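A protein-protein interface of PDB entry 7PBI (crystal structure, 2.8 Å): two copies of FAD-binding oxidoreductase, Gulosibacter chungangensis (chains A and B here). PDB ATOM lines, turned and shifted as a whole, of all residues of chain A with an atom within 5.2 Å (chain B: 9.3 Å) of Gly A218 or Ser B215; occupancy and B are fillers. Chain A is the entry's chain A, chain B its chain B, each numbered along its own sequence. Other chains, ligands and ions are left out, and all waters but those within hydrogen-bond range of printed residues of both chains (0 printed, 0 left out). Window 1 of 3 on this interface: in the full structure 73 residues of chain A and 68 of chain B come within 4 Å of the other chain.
Of the 20 printed residues of chain B, 5 touch a printed residue of chain A.
Hydrophobic or aromatic side chains of chain B within 4 Å of the printed part of chain A: Tyr B208, Pro B214 and Leu B219.
Of the 8 printed residues of chain A, 4 touch a printed residue of chain B.
Among the printed residues, no Asp or Glu carboxylate lies within 4 Å of a Lys or Arg side-chain nitrogen of the other chain.
Leu B219 touches its own counterpart, Leu A219.
6 positions are printed for both chains.
Pro B214 touches Gly A218.
O of Gly A218 touches O of Ser B215, 3.9 Å away.
Pro B214 touches Leu A219 (CB to O, 3.5 Å).
Ser B215 touches Leu A219 (O to CD2, 3.96 Å).
CD2 of Leu A219 touches CD1 of Leu B219, 3.96 Å away.
Glu A221 touches Gly B213 (O to C, 3.4 Å).
Of chain B, only Pro B214 and Ser B215 come within 4 Å of Gly A218.
Ser B215 touches just these residues of chain A: Gly A218 (3.9 Å) and Leu A219 (3.96 Å).
Printed residues of chain A within 4 Å of Gly B213: Glu A221.
Of the printed residues of chain A, Leu B219 touches Leu A219 (3.96 Å).
Of the printed residues of chain B, Glu A221 touches Gly B213 and Pro B214.
Of the printed residues of chain B, His A165 touches Tyr B208.
Cys B180 touches none of the printed residues of chain A.
Glu A217 touches none of the printed residues of chain B.
The nearest residue of chain B that does not touch Gly A218 is Gly B213 (5.9 Å).
The nearest residue of chain A that does not touch Ser B215 is His A165 (5.0 Å).
The nearest printed residue of chain B that does not touch Leu A219 is Ile B216 (4.2 Å).
The backbone carbonyl oxygen of Pro B214 is in hydrogen-bond range of the side-chain amide nitrogen of Gln B211 (3.2 Å).
OE1 of Gln B211 lies within hydrogen-bond range of OG of Ser B215 (3.4 Å).
O of Pro B209 lies within hydrogen-bond range of OG of Ser B215, 3.3 Å away.
The backbone NH of Tyr B208 lies close to the side-chain sulfur of Cys B180.
NH1 of Arg A179 is in salt-bridge range of OE2 of Glu A221 (2.6 Å).
The backbone carbonyl oxygen (O) of Glu A221 sits close to the backbone nitrogen (N) of Pro B214 (3.3 Å).
A ring nitrogen (ND1) of His A165 lies within hydrogen-bond range of the side-chain hydroxyl (OH) of Tyr B208.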
ATOM      1  N   HIS A 165     -20.256  17.320  13.066  1.00  0.00           N
ATOM      2  CA  HIS A 165     -19.667  17.936  11.851  1.00  0.00           C
ATOM      3  C   HIS A 165     -20.190  19.378  11.782  1.00  0.00           C
ATOM      4  O   HIS A 165     -20.475  19.896  10.671  1.00  0.00           O
ATOM      5  CB  HIS A 165     -20.018  17.089  10.618  1.00  0.00           C
ATOM      6  CG  HIS A 165     -18.913  16.953   9.630  1.00  0.00           C
ATOM      7  ND1 HIS A 165     -18.638  17.933   8.688  1.00  0.00           N
ATOM      8  CD2 HIS A 165     -18.023  15.958   9.418  1.00  0.00           C
ATOM      9  CE1 HIS A 165     -17.613  17.556   7.947  1.00  0.00           C
ATOM     10  NE2 HIS A 165     -17.221  16.342   8.372  1.00  0.00           N
ATOM     11  N   ARG A 179     -10.355  19.577  15.659  1.00  0.00           N
ATOM     12  CA  ARG A 179     -10.336  18.601  16.777  1.00  0.00           C
ATOM     13  C   ARG A 179      -9.134  17.696  16.522  1.00  0.00           C
ATOM     14  O   ARG A 179      -8.864  17.398  15.354  1.00  0.00           O
ATOM     15  CB  ARG A 179     -11.599  17.742  16.864  1.00  0.00           C
ATOM     16  CG  ARG A 179     -11.349  16.325  16.382  1.00  0.00           C
ATOM     17  CD  ARG A 179     -12.533  15.644  15.777  1.00  0.00           C
ATOM     18  NE  ARG A 179     -11.966  14.893  14.678  1.00  0.00           N
ATOM     19  CZ  ARG A 179     -12.658  14.178  13.818  1.00  0.00           C
ATOM     20  NH1 ARG A 179     -13.975  14.059  13.945  1.00  0.00           N
ATOM     21  NH2 ARG A 179     -12.013  13.539  12.860  1.00  0.00           N
ATOM     22  N   ILE A 216      -9.217   6.780  12.943  1.00  0.00           N
ATOM     23  CA  ILE A 216     -10.639   6.420  13.177  1.00  0.00           C
ATOM     24  C   ILE A 216     -11.373   7.564  13.886  1.00  0.00           C
ATOM     25  O   ILE A 216     -12.548   7.359  14.227  1.00  0.00           O
ATOM     26  CB  ILE A 216     -10.709   5.104  13.964  1.00  0.00           C
ATOM     27  CG1 ILE A 216     -10.508   5.301  15.466  1.00  0.00           C
ATOM     28  CG2 ILE A 216      -9.712   4.106  13.399  1.00  0.00           C
ATOM     29  CD1 ILE A 216     -10.787   4.051  16.251  1.00  0.00           C
ATOM     30  N   GLU A 217     -10.729   8.715  14.106  1.00  0.00           N
ATOM     31  CA  GLU A 217     -11.367   9.886  14.769  1.00  0.00           C
ATOM     32  C   GLU A 217     -12.628  10.267  13.997  1.00  0.00           C
ATOM     33  O   GLU A 217     -13.660  10.539  14.630  1.00  0.00           O
ATOM     34  CB  GLU A 217     -10.440  11.100  14.808  1.00  0.00           C
ATOM     35  CG  GLU A 217      -9.451  11.085  15.962  1.00  0.00           C
ATOM     36  CD  GLU A 217      -8.939  12.454  16.375  1.00  0.00           C
ATOM     37  OE1 GLU A 217      -9.508  13.484  15.925  1.00  0.00           O
ATOM     38  OE2 GLU A 217      -7.966  12.487  17.145  1.00  0.00           O
ATOM     39  N   GLY A 218     -12.525  10.284  12.671  1.00  0.00           N
ATOM     40  CA  GLY A 218     -13.629  10.620  11.760  1.00  0.00           C
ATOM     41  C   GLY A 218     -14.774   9.640  11.871  1.00  0.00           C
ATOM     42  O   GLY A 218     -15.884  10.021  11.488  1.00  0.00           O
ATOM     43  N   LEU A 219     -14.517   8.420  12.346  1.00  0.00           N
ATOM     44  CA  LEU A 219     -15.560   7.371  12.506  1.00  0.00           C
ATOM     45  C   LEU A 219     -16.569   7.795  13.579  1.00  0.00           C
ATOM     46  O   LEU A 219     -17.712   7.285  13.520  1.00  0.00           O
ATOM     47  CB  LEU A 219     -14.939   6.027  12.904  1.00  0.00           C
ATOM     48  CG  LEU A 219     -14.310   5.191  11.796  1.00  0.00           C
ATOM     49  CD1 LEU A 219     -13.998   3.794  12.314  1.00  0.00           C
ATOM     50  CD2 LEU A 219     -15.229   5.114  10.588  1.00  0.00           C
ATOM     51  N   PHE A 220     -16.170   8.650  14.533  1.00  0.00           N
ATOM     52  CA  PHE A 220     -17.026   9.050  15.682  1.00  0.00           C
ATOM     53  C   PHE A 220     -17.844  10.304  15.341  1.00  0.00           C
ATOM     54  O   PHE A 220     -18.148  11.108  16.258  1.00  0.00           O
ATOM     55  CB  PHE A 220     -16.177   9.261  16.936  1.00  0.00           C
ATOM     56  CG  PHE A 220     -15.526   8.000  17.427  1.00  0.00           C
ATOM     57  CD1 PHE A 220     -16.298   6.953  17.891  1.00  0.00           C
ATOM     58  CD2 PHE A 220     -14.151   7.842  17.386  1.00  0.00           C
ATOM     59  CE1 PHE A 220     -15.710   5.774  18.317  1.00  0.00           C
ATOM     60  CE2 PHE A 220     -13.561   6.662  17.817  1.00  0.00           C
ATOM     61  CZ  PHE A 220     -14.343   5.632  18.280  1.00  0.00           C
ATOM     62  N   GLU A 221     -18.232  10.479  14.074  1.00  0.00           N
ATOM     63  CA  GLU A 221     -19.023  11.675  13.697  1.00  0.00           C
ATOM     64  C   GLU A 221     -20.358  11.290  13.073  1.00  0.00           C
ATOM     65  O   GLU A 221     -20.398  10.453  12.160  1.00  0.00           O
ATOM     66  CB  GLU A 221     -18.187  12.609  12.841  1.00  0.00           C
ATOM     67  CG  GLU A 221     -17.218  13.349  13.718  1.00  0.00           C
ATOM     68  CD  GLU A 221     -16.853  14.718  13.216  1.00  0.00           C
ATOM     69  OE1 GLU A 221     -17.202  15.029  12.041  1.00  0.00           O
ATOM     70  OE2 GLU A 221     -16.218  15.457  14.006  1.00  0.00           O
ATOM     71  N   ARG B 179      -7.394  15.047  -0.783  1.00  0.00           N
ATOM     72  CA  ARG B 179      -8.168  13.904  -1.329  1.00  0.00           C
ATOM     73  C   ARG B 179      -9.657  14.174  -1.085  1.00  0.00           C
ATOM     74  O   ARG B 179     -10.000  14.603   0.015  1.00  0.00           O
ATOM     75  CB  ARG B 179      -7.715  12.619  -0.643  1.00  0.00           C
ATOM     76  CG  ARG B 179      -8.644  11.438  -0.863  1.00  0.00           C
ATOM     77  CD  ARG B 179      -8.481  10.430   0.260  1.00  0.00           C
ATOM     78  NE  ARG B 179      -9.236  10.787   1.462  1.00  0.00           N
ATOM     79  CZ  ARG B 179      -8.742  10.933   2.685  1.00  0.00           C
ATOM     80  NH1 ARG B 179      -7.461  10.741   2.934  1.00  0.00           N
ATOM     81  NH2 ARG B 179      -9.559  11.260   3.667  1.00  0.00           N
ATOM     82  N   CYS B 180     -10.514  13.964  -2.074  1.00  0.00           N
ATOM     83  CA  CYS B 180     -11.985  14.128  -1.933  1.00  0.00           C
ATOM     84  C   CYS B 180     -12.686  13.284  -2.998  1.00  0.00           C
ATOM     85  O   CYS B 180     -12.591  13.629  -4.196  1.00  0.00           O
ATOM     86  CB  CYS B 180     -12.418  15.592  -2.020  1.00  0.00           C
ATOM     87  SG  CYS B 180     -14.121  15.891  -1.451  1.00  0.00           S
ATOM     88  N   GLY B 181     -13.323  12.200  -2.555  1.00  0.00           N
ATOM     89  CA  GLY B 181     -14.179  11.334  -3.381  1.00  0.00           C
ATOM     90  C   GLY B 181     -13.406  10.156  -3.923  1.00  0.00           C
ATOM     91  O   GLY B 181     -12.679  10.334  -4.907  1.00  0.00           O
ATOM     92  N   LEU B 192     -17.742   0.721  -3.637  1.00  0.00           N
ATOM     93  CA  LEU B 192     -18.220   1.821  -2.754  1.00  0.00           C
ATOM     94  C   LEU B 192     -17.804   3.142  -3.385  1.00  0.00           C
ATOM     95  O   LEU B 192     -16.688   3.188  -3.940  1.00  0.00           O
ATOM     96  CB  LEU B 192     -17.612   1.664  -1.358  1.00  0.00           C
ATOM     97  CG  LEU B 192     -17.770   2.860  -0.423  1.00  0.00           C
ATOM     98  CD1 LEU B 192     -19.150   2.902   0.207  1.00  0.00           C
ATOM     99  CD2 LEU B 192     -16.712   2.829   0.662  1.00  0.00           C
ATOM    100  N   THR B 194     -17.378   7.024  -1.961  1.00  0.00           N
ATOM    101  CA  THR B 194     -17.262   7.698  -0.647  1.00  0.00           C
ATOM    102  C   THR B 194     -18.016   9.030  -0.681  1.00  0.00           C
ATOM    103  O   THR B 194     -18.230   9.580  -1.763  1.00  0.00           O
ATOM    104  CB  THR B 194     -15.795   7.863  -0.250  1.00  0.00           C
ATOM    105  OG1 THR B 194     -15.189   8.742  -1.201  1.00  0.00           O
ATOM    106  CG2 THR B 194     -15.084   6.529  -0.189  1.00  0.00           C
ATOM    107  N   GLY B 195     -18.428   9.502   0.489  1.00  0.00           N
ATOM    108  CA  GLY B 195     -19.062  10.819   0.664  1.00  0.00           C
ATOM    109  C   GLY B 195     -20.186  11.011  -0.329  1.00  0.00           C
ATOM    110  O   GLY B 195     -20.982  10.077  -0.497  1.00  0.00           O
ATOM    111  N   MET B 196     -20.203  12.154  -1.014  1.00  0.00           N
ATOM    112  CA  MET B 196     -21.334  12.593  -1.867  1.00  0.00           C
ATOM    113  C   MET B 196     -21.388  11.751  -3.144  1.00  0.00           C
ATOM    114  O   MET B 196     -22.383  11.868  -3.894  1.00  0.00           O
ATOM    115  CB  MET B 196     -21.201  14.072  -2.227  1.00  0.00           C
ATOM    116  CG  MET B 196     -21.367  14.988  -1.045  1.00  0.00           C
ATOM    117  SD  MET B 196     -23.067  15.005  -0.475  1.00  0.00           S
ATOM    118  CE  MET B 196     -22.920  16.176   0.872  1.00  0.00           C
ATOM    119  N   TYR B 208     -16.982  18.214  -1.314  1.00  0.00           N
ATOM    120  CA  TYR B 208     -17.177  18.161   0.159  1.00  0.00           C
ATOM    121  C   TYR B 208     -16.910  16.736   0.637  1.00  0.00           C
ATOM    122  O   TYR B 208     -17.653  15.807   0.303  1.00  0.00           O
ATOM    123  CB  TYR B 208     -18.565  18.682   0.542  1.00  0.00           C
ATOM    124  CG  TYR B 208     -18.912  18.600   2.011  1.00  0.00           C
ATOM    125  CD1 TYR B 208     -18.308  19.426   2.951  1.00  0.00           C
ATOM    126  CD2 TYR B 208     -19.874  17.709   2.464  1.00  0.00           C
ATOM    127  CE1 TYR B 208     -18.638  19.353   4.299  1.00  0.00           C
ATOM    128  CE2 TYR B 208     -20.212  17.619   3.806  1.00  0.00           C
ATOM    129  CZ  TYR B 208     -19.592  18.441   4.734  1.00  0.00           C
ATOM    130  OH  TYR B 208     -19.922  18.340   6.063  1.00  0.00           O
ATOM    131  N   PRO B 209     -15.840  16.530   1.443  1.00  0.00           N
ATOM    132  CA  PRO B 209     -15.484  15.208   1.941  1.00  0.00           C
ATOM    133  C   PRO B 209     -16.421  14.839   3.093  1.00  0.00           C
ATOM    134  O   PRO B 209     -15.962  14.675   4.212  1.00  0.00           O
ATOM    135  CB  PRO B 209     -14.043  15.407   2.414  1.00  0.00           C
ATOM    136  CG  PRO B 209     -14.052  16.820   2.941  1.00  0.00           C
ATOM    137  CD  PRO B 209     -14.937  17.570   1.967  1.00  0.00           C
ATOM    138  N   GLY B 210     -17.710  14.725   2.778  1.00  0.00           N
ATOM    139  CA  GLY B 210     -18.761  14.513   3.782  1.00  0.00           C
ATOM    140  C   GLY B 210     -20.038  13.974   3.176  1.00  0.00           C
ATOM    141  O   GLY B 210     -20.167  13.952   1.931  1.00  0.00           O
ATOM    142  N   GLN B 211     -20.943  13.573   4.066  1.00  0.00           N
ATOM    143  CA  GLN B 211     -22.227  12.889   3.782  1.00  0.00           C
ATOM    144  C   GLN B 211     -22.889  12.668   5.138  1.00  0.00           C
ATOM    145  O   GLN B 211     -22.235  12.955   6.155  1.00  0.00           O
ATOM    146  CB  GLN B 211     -21.999  11.579   3.019  1.00  0.00           C
ATOM    147  CG  GLN B 211     -21.527  10.403   3.870  1.00  0.00           C
ATOM    148  CD  GLN B 211     -20.100  10.494   4.353  1.00  0.00           C
ATOM    149  OE1 GLN B 211     -19.654  11.509   4.887  1.00  0.00           O
ATOM    150  NE2 GLN B 211     -19.373   9.399   4.186  1.00  0.00           N
ATOM    151  N   LEU B 212     -24.131  12.198   5.154  1.00  0.00           N
ATOM    152  CA  LEU B 212     -24.802  11.824   6.421  1.00  0.00           C
ATOM    153  C   LEU B 212     -24.050  10.639   7.029  1.00  0.00           C
ATOM    154  O   LEU B 212     -23.888   9.616   6.324  1.00  0.00           O
ATOM    155  CB  LEU B 212     -26.266  11.463   6.165  1.00  0.00           C
ATOM    156  CG  LEU B 212     -27.118  11.407   7.431  1.00  0.00           C
ATOM    157  CD1 LEU B 212     -27.608  12.796   7.794  1.00  0.00           C
ATOM    158  CD2 LEU B 212     -28.277  10.442   7.272  1.00  0.00           C
ATOM    159  N   GLY B 213     -23.621  10.781   8.287  1.00  0.00           N
ATOM    160  CA  GLY B 213     -22.918   9.724   9.039  1.00  0.00           C
ATOM    161  C   GLY B 213     -21.405   9.859   8.931  1.00  0.00           C
ATOM    162  O   GLY B 213     -20.905  10.867   8.451  1.00  0.00           O
ATOM    163  N   PRO B 214     -20.626   8.836   9.349  1.00  0.00           N
ATOM    164  CA  PRO B 214     -19.174   8.964   9.441  1.00  0.00           C
ATOM    165  C   PRO B 214     -18.570   9.017   8.038  1.00  0.00           C
ATOM    166  O   PRO B 214     -19.091   8.354   7.153  1.00  0.00           O
ATOM    167  CB  PRO B 214     -18.704   7.687  10.151  1.00  0.00           C
ATOM    168  CG  PRO B 214     -19.979   6.980  10.596  1.00  0.00           C
ATOM    169  CD  PRO B 214     -21.086   7.484   9.695  1.00  0.00           C
ATOM    170  N   SER B 215     -17.508   9.797   7.858  1.00  0.00           N
ATOM    171  CA  SER B 215     -16.608   9.650   6.685  1.00  0.00           C
ATOM    172  C   SER B 215     -15.781   8.382   6.914  1.00  0.00           C
ATOM    173  O   SER B 215     -15.350   8.164   8.063  1.00  0.00           O
ATOM    174  CB  SER B 215     -15.737  10.863   6.463  1.00  0.00           C
ATOM    175  OG  SER B 215     -16.507  11.999   6.095  1.00  0.00           O
ATOM    176  N   ILE B 216     -15.612   7.552   5.886  1.00  0.00           N
ATOM    177  CA  ILE B 216     -14.740   6.340   5.959  1.00  0.00           C
ATOM    178  C   ILE B 216     -13.550   6.475   5.003  1.00  0.00           C
ATOM    179  O   ILE B 216     -12.729   5.553   4.983  1.00  0.00           O
ATOM    180  CB  ILE B 216     -15.542   5.054   5.706  1.00  0.00           C
ATOM    181  CG1 ILE B 216     -16.027   4.944   4.260  1.00  0.00           C
ATOM    182  CG2 ILE B 216     -16.683   4.953   6.704  1.00  0.00           C
ATOM    183  CD1 ILE B 216     -16.847   3.699   3.990  1.00  0.00           C
ATOM    184  N   GLU B 217     -13.414   7.587   4.278  1.00  0.00           N
ATOM    185  CA  GLU B 217     -12.212   7.819   3.435  1.00  0.00           C
ATOM    186  C   GLU B 217     -10.950   7.588   4.283  1.00  0.00           C
ATOM    187  O   GLU B 217     -10.014   6.946   3.772  1.00  0.00           O
ATOM    188  CB  GLU B 217     -12.249   9.207   2.801  1.00  0.00           C
ATOM    189  CG  GLU B 217     -13.031   9.231   1.504  1.00  0.00           C
ATOM    190  CD  GLU B 217     -12.901  10.504   0.679  1.00  0.00           C
ATOM    191  OE1 GLU B 217     -11.985  11.312   0.952  1.00  0.00           O
ATOM    192  OE2 GLU B 217     -13.740  10.701  -0.229  1.00  0.00           O
ATOM    193  N   GLY B 218     -10.964   8.032   5.544  1.00  0.00           N
ATOM    194  CA  GLY B 218      -9.833   7.932   6.481  1.00  0.00           C
ATOM    195  C   GLY B 218      -9.362   6.502   6.667  1.00  0.00           C
ATOM    196  O   GLY B 218      -8.160   6.317   6.929  1.00  0.00           O
ATOM    197  N   LEU B 219     -10.257   5.520   6.521  1.00  0.00           N
ATOM    198  CA  LEU B 219      -9.974   4.083   6.810  1.00  0.00           C
ATOM    199  C   LEU B 219      -9.038   3.454   5.767  1.00  0.00           C
ATOM    200  O   LEU B 219      -8.378   2.447   6.101  1.00  0.00           O
ATOM    201  CB  LEU B 219     -11.287   3.302   6.842  1.00  0.00           C
ATOM    202  CG  LEU B 219     -12.164   3.530   8.065  1.00  0.00           C
ATOM    203  CD1 LEU B 219     -13.484   2.791   7.903  1.00  0.00           C
ATOM    204  CD2 LEU B 219     -11.445   3.078   9.324  1.00  0.00           C
ATOM    205  N   PHE B 220      -8.987   3.980   4.543  1.00  0.00           N
ATOM    206  CA  PHE B 220      -8.229   3.341   3.438  1.00  0.00           C
ATOM    207  C   PHE B 220      -6.793   3.868   3.404  1.00  0.00           C
ATOM    208  O   PHE B 220      -6.113   3.675   2.372  1.00  0.00           O
ATOM    209  CB  PHE B 220      -8.970   3.537   2.121  1.00  0.00           C
ATOM    210  CG  PHE B 220     -10.386   3.031   2.171  1.00  0.00           C
ATOM    211  CD1 PHE B 220     -10.656   1.674   2.248  1.00  0.00           C
ATOM    212  CD2 PHE B 220     -11.448   3.915   2.166  1.00  0.00           C
ATOM    213  CE1 PHE B 220     -11.960   1.208   2.305  1.00  0.00           C
ATOM    214  CE2 PHE B 220     -12.752   3.445   2.211  1.00  0.00           C
ATOM    215  CZ  PHE B 220     -13.007   2.097   2.295  1.00  0.00           C
